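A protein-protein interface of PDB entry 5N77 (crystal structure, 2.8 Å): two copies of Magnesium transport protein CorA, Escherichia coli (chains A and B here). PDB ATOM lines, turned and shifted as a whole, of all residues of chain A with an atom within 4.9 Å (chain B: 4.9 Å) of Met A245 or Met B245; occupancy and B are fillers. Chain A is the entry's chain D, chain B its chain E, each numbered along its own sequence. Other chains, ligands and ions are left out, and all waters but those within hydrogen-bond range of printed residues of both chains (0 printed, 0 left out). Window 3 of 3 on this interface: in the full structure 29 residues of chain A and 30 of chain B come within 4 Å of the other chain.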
ATOM      1  N   MET A 241      -3.817   5.062 -29.951  1.00  0.00           N
ATOM      2  CA  MET A 241      -2.778   4.832 -28.976  1.00  0.00           C
ATOM      3  C   MET A 241      -3.187   5.394 -27.614  1.00  0.00           C
ATOM      4  O   MET A 241      -3.031   4.764 -26.584  1.00  0.00           O
ATOM      5  CB  MET A 241      -1.498   5.500 -29.465  1.00  0.00           C
ATOM      6  CG  MET A 241      -0.261   5.269 -28.614  1.00  0.00           C
ATOM      7  SD  MET A 241       0.148   3.525 -28.420  1.00  0.00           S
ATOM      8  CE  MET A 241       0.614   3.243 -30.125  1.00  0.00           C
ATOM      9  N   GLN A 242      -3.760   6.583 -27.618  1.00  0.00           N
ATOM     10  CA  GLN A 242      -4.174   7.235 -26.381  1.00  0.00           C
ATOM     11  C   GLN A 242      -5.300   6.473 -25.706  1.00  0.00           C
ATOM     12  O   GLN A 242      -5.320   6.342 -24.492  1.00  0.00           O
ATOM     13  CB  GLN A 242      -4.600   8.706 -26.626  1.00  0.00           C
ATOM     14  CG  GLN A 242      -3.468   9.723 -26.617  1.00  0.00           C
ATOM     15  CD  GLN A 242      -2.405   9.439 -25.554  1.00  0.00           C
ATOM     16  OE1 GLN A 242      -2.681   9.493 -24.346  1.00  0.00           O
ATOM     17  NE2 GLN A 242      -1.174   9.127 -26.004  1.00  0.00           N
ATOM     18  N   ALA A 243      -6.264   6.024 -26.493  1.00  0.00           N
ATOM     19  CA  ALA A 243      -7.441   5.373 -25.940  1.00  0.00           C
ATOM     20  C   ALA A 243      -7.023   4.055 -25.299  1.00  0.00           C
ATOM     21  O   ALA A 243      -7.498   3.675 -24.210  1.00  0.00           O
ATOM     22  CB  ALA A 243      -8.466   5.134 -27.026  1.00  0.00           C
ATOM     23  N   ALA A 244      -6.125   3.362 -25.980  1.00  0.00           N
ATOM     24  CA  ALA A 244      -5.580   2.102 -25.477  1.00  0.00           C
ATOM     25  C   ALA A 244      -4.946   2.261 -24.116  1.00  0.00           C
ATOM     26  O   ALA A 244      -5.192   1.459 -23.208  1.00  0.00           O
ATOM     27  CB  ALA A 244      -4.564   1.571 -26.451  1.00  0.00           C
ATOM     28  N   MET A 245      -4.149   3.313 -23.956  1.00  0.00           N
ATOM     29  CA  MET A 245      -3.518   3.572 -22.672  1.00  0.00           C
ATOM     30  C   MET A 245      -4.563   3.829 -21.620  1.00  0.00           C
ATOM     31  O   MET A 245      -4.409   3.425 -20.475  1.00  0.00           O
ATOM     32  CB  MET A 245      -2.489   4.686 -22.748  1.00  0.00           C
ATOM     33  CG  MET A 245      -1.231   4.218 -23.489  1.00  0.00           C
ATOM     34  SD  MET A 245       0.054   5.454 -23.770  1.00  0.00           S
ATOM     35  CE  MET A 245       0.641   5.631 -22.076  1.00  0.00           C
ATOM     36  N   GLY A 246      -5.663   4.442 -22.019  1.00  0.00           N
ATOM     37  CA  GLY A 246      -6.779   4.648 -21.093  1.00  0.00           C
ATOM     38  C   GLY A 246      -7.396   3.344 -20.595  1.00  0.00           C
ATOM     39  O   GLY A 246      -7.706   3.184 -19.415  1.00  0.00           O
ATOM     40  N   PHE A 247      -7.586   2.420 -21.523  1.00  0.00           N
ATOM     41  CA  PHE A 247      -8.161   1.129 -21.203  1.00  0.00           C
ATOM     42  C   PHE A 247      -7.210   0.295 -20.357  1.00  0.00           C
ATOM     43  O   PHE A 247      -7.634  -0.391 -19.424  1.00  0.00           O
ATOM     44  CB  PHE A 247      -8.558   0.403 -22.471  1.00  0.00           C
ATOM     45  CG  PHE A 247      -9.792   0.960 -23.102  1.00  0.00           C
ATOM     46  CD1 PHE A 247     -10.989   0.971 -22.411  1.00  0.00           C
ATOM     47  CD2 PHE A 247      -9.759   1.485 -24.389  1.00  0.00           C
ATOM     48  CE1 PHE A 247     -12.122   1.494 -22.982  1.00  0.00           C
ATOM     49  CE2 PHE A 247     -10.907   2.019 -24.970  1.00  0.00           C
ATOM     50  CZ  PHE A 247     -12.086   2.024 -24.256  1.00  0.00           C
ATOM     51  N   ILE A 248      -5.927   0.371 -20.677  1.00  0.00           N
ATOM     52  CA  ILE A 248      -4.901  -0.280 -19.881  1.00  0.00           C
ATOM     53  C   ILE A 248      -4.844   0.252 -18.459  1.00  0.00           C
ATOM     54  O   ILE A 248      -4.567  -0.502 -17.546  1.00  0.00           O
ATOM     55  CB  ILE A 248      -3.517  -0.105 -20.530  1.00  0.00           C
ATOM     56  CG1 ILE A 248      -3.412  -0.938 -21.808  1.00  0.00           C
ATOM     57  CG2 ILE A 248      -2.400  -0.526 -19.597  1.00  0.00           C
ATOM     58  CD1 ILE A 248      -2.381  -0.382 -22.766  1.00  0.00           C
ATOM     59  N   ASN A 249      -5.067   1.545 -18.274  1.00  0.00           N
ATOM     60  CA  ASN A 249      -5.056   2.126 -16.928  1.00  0.00           C
ATOM     61  C   ASN A 249      -6.332   1.809 -16.197  1.00  0.00           C
ATOM     62  O   ASN A 249      -6.338   1.742 -14.972  1.00  0.00           O
ATOM     63  CB  ASN A 249      -4.931   3.644 -16.944  1.00  0.00           C
ATOM     64  CG  ASN A 249      -3.517   4.140 -17.160  1.00  0.00           C
ATOM     65  OD1 ASN A 249      -3.311   5.355 -17.225  1.00  0.00           O
ATOM     66  ND2 ASN A 249      -2.545   3.242 -17.299  1.00  0.00           N
ATOM     67  N   MET B 241      -9.963  12.990 -23.556  1.00  0.00           N
ATOM     68  CA  MET B 241      -9.199  11.785 -23.394  1.00  0.00           C
ATOM     69  C   MET B 241      -8.113  12.002 -22.335  1.00  0.00           C
ATOM     70  O   MET B 241      -7.892  11.161 -21.473  1.00  0.00           O
ATOM     71  CB  MET B 241      -8.582  11.417 -24.745  1.00  0.00           C
ATOM     72  CG  MET B 241      -7.821  10.105 -24.802  1.00  0.00           C
ATOM     73  SD  MET B 241      -8.834   8.700 -24.330  1.00  0.00           S
ATOM     74  CE  MET B 241      -9.914   8.754 -25.762  1.00  0.00           C
ATOM     75  N   GLN B 242      -7.435  13.137 -22.399  1.00  0.00           N
ATOM     76  CA  GLN B 242      -6.349  13.419 -21.483  1.00  0.00           C
ATOM     77  C   GLN B 242      -6.847  13.589 -20.061  1.00  0.00           C
ATOM     78  O   GLN B 242      -6.226  13.117 -19.126  1.00  0.00           O
ATOM     79  CB  GLN B 242      -5.562  14.678 -21.902  1.00  0.00           C
ATOM     80  CG  GLN B 242      -4.451  14.438 -22.927  1.00  0.00           C
ATOM     81  CD  GLN B 242      -3.681  13.118 -22.705  1.00  0.00           C
ATOM     82  OE1 GLN B 242      -2.994  12.956 -21.673  1.00  0.00           O
ATOM     83  NE2 GLN B 242      -3.785  12.183 -23.670  1.00  0.00           N
ATOM     84  N   ALA B 243      -7.956  14.281 -19.906  1.00  0.00           N
ATOM     85  CA  ALA B 243      -8.518  14.564 -18.582  1.00  0.00           C
ATOM     86  C   ALA B 243      -8.969  13.265 -17.908  1.00  0.00           C
ATOM     87  O   ALA B 243      -8.708  13.049 -16.721  1.00  0.00           O
ATOM     88  CB  ALA B 243      -9.696  15.503 -18.695  1.00  0.00           C
ATOM     89  N   ALA B 244      -9.589  12.393 -18.705  1.00  0.00           N
ATOM     90  CA  ALA B 244      -9.999  11.088 -18.251  1.00  0.00           C
ATOM     91  C   ALA B 244      -8.829  10.292 -17.679  1.00  0.00           C
ATOM     92  O   ALA B 244      -8.939   9.701 -16.597  1.00  0.00           O
ATOM     93  CB  ALA B 244     -10.626  10.331 -19.386  1.00  0.00           C
ATOM     94  N   MET B 245      -7.703  10.281 -18.390  1.00  0.00           N
ATOM     95  CA  MET B 245      -6.540   9.552 -17.912  1.00  0.00           C
ATOM     96  C   MET B 245      -6.071  10.150 -16.623  1.00  0.00           C
ATOM     97  O   MET B 245      -5.595   9.429 -15.735  1.00  0.00           O
ATOM     98  CB  MET B 245      -5.433   9.483 -18.956  1.00  0.00           C
ATOM     99  CG  MET B 245      -5.806   8.509 -20.075  1.00  0.00           C
ATOM    100  SD  MET B 245      -4.684   8.405 -21.472  1.00  0.00           S
ATOM    101  CE  MET B 245      -3.324   7.557 -20.655  1.00  0.00           C
ATOM    102  N   GLY B 246      -6.232  11.457 -16.480  1.00  0.00           N
ATOM    103  CA  GLY B 246      -5.852  12.134 -15.228  1.00  0.00           C
ATOM    104  C   GLY B 246      -6.687  11.683 -14.064  1.00  0.00           C
ATOM    105  O   GLY B 246      -6.174  11.434 -12.966  1.00  0.00           O
ATOM    106  N   PHE B 247      -7.982  11.547 -14.323  1.00  0.00           N
ATOM    107  CA  PHE B 247      -8.910  11.136 -13.307  1.00  0.00           C
ATOM    108  C   PHE B 247      -8.737   9.673 -12.929  1.00  0.00           C
ATOM    109  O   PHE B 247      -8.773   9.332 -11.748  1.00  0.00           O
ATOM    110  CB  PHE B 247     -10.326  11.409 -13.761  1.00  0.00           C
ATOM    111  CG  PHE B 247     -10.667  12.850 -13.745  1.00  0.00           C
ATOM    112  CD1 PHE B 247     -10.496  13.595 -12.600  1.00  0.00           C
ATOM    113  CD2 PHE B 247     -11.171  13.471 -14.853  1.00  0.00           C
ATOM    114  CE1 PHE B 247     -10.812  14.938 -12.565  1.00  0.00           C
ATOM    115  CE2 PHE B 247     -11.479  14.823 -14.826  1.00  0.00           C
ATOM    116  CZ  PHE B 247     -11.301  15.559 -13.688  1.00  0.00           C
ATOM    117  N   ILE B 248      -8.502   8.837 -13.928  1.00  0.00           N
ATOM    118  CA  ILE B 248      -8.149   7.439 -13.713  1.00  0.00           C
ATOM    119  C   ILE B 248      -6.879   7.272 -12.857  1.00  0.00           C
ATOM    120  O   ILE B 248      -6.801   6.347 -12.074  1.00  0.00           O
ATOM    121  CB  ILE B 248      -7.935   6.716 -15.062  1.00  0.00           C
ATOM    122  CG1 ILE B 248      -9.254   6.540 -15.799  1.00  0.00           C
ATOM    123  CG2 ILE B 248      -7.332   5.358 -14.857  1.00  0.00           C
ATOM    124  CD1 ILE B 248      -9.074   6.402 -17.294  1.00  0.00           C
ATOM    125  N   ASN B 249      -5.877   8.135 -13.032  1.00  0.00           N
ATOM    126  CA  ASN B 249      -4.644   8.041 -12.242  1.00  0.00           C
ATOM    127  C   ASN B 249      -4.824   8.587 -10.859  1.00  0.00           C
ATOM    128  O   ASN B 249      -4.145   8.161  -9.923  1.00  0.00           O
ATOM    129  CB  ASN B 249      -3.495   8.827 -12.874  1.00  0.00           C
ATOM    130  CG  ASN B 249      -2.830   8.122 -14.037  1.00  0.00           C
ATOM    131  OD1 ASN B 249      -1.888   8.669 -14.616  1.00  0.00           O
ATOM    132  ND2 ASN B 249      -3.277   6.916 -14.380  1.00  0.00           N
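Gln A242 touches Met B241, but with the chains exchanged Met A241 does not touch Gln B242 (7.9 Å). Gln A242 touches Met B245, but with the chains exchanged Met A245 does not touch Gln B242 (7.7 Å). Ala A243 touches Met B241, but with the chains exchanged Met A241 does not touch Ala B243 (12.6 Å). Met A245 touches its own counterpart, Met B245. Of the 7 pairs that touch across the chains among the printed residues, 3 have their exchanged pair printed and touching as well.
CG of Met B241 touches CB of Gln A242, at 3.96 Å. Met B241 touches Ala A243. Met B245 touches Met A245. Ile B248 touches Asn A249.
NE2 of Gln B242 is in hydrogen-bond range of OE1 of Gln A242, 3.0 Å away. OE1 of Gln A242 lies close to SD of Met B245 (3.7 Å). ND2 of Asn B249 lies within hydrogen-bond range of OD1 of Asn A249 (3.2 Å).
Met A245 touches just one residue of chain B: Met B245. Met B245 touches two residues of chain A. Printed residues of chain A within 4 Å of Met B241: Gln A242 and Ala A243. Of the printed residues of chain B, Gln A242 touches Met B241 (3.96 Å), Gln B242 (3.0 Å) and Met B245 (3.7 Å). Printed residues of chain B within 4 Å of Asn A249: Ile B248 and Asn B249. Printed residues of chain B within 4 Å of Ala A243: Met B241. The nearest residue of chain A that does not touch Met B245 is Asn A249 (4.1 Å).
Of the 9 printed residues of chain B, 5 touch a printed residue of chain A. Printed residues of chain B that touch a printed residue of chain A: Met B241, Gln B242, Met B245, Ile B248 and Asn B249. Hydrophobic or aromatic side chains of chain B within 4 Å of the printed part of chain A: Met B241, Met B245 and Ile B248. Of the 9 printed residues of chain A, 4 touch a printed residue of chain B. Among the printed residues, no Asp or Glu carboxylate lies within 4 Å of a Lys or Arg side-chain nitrogen of the other chain.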
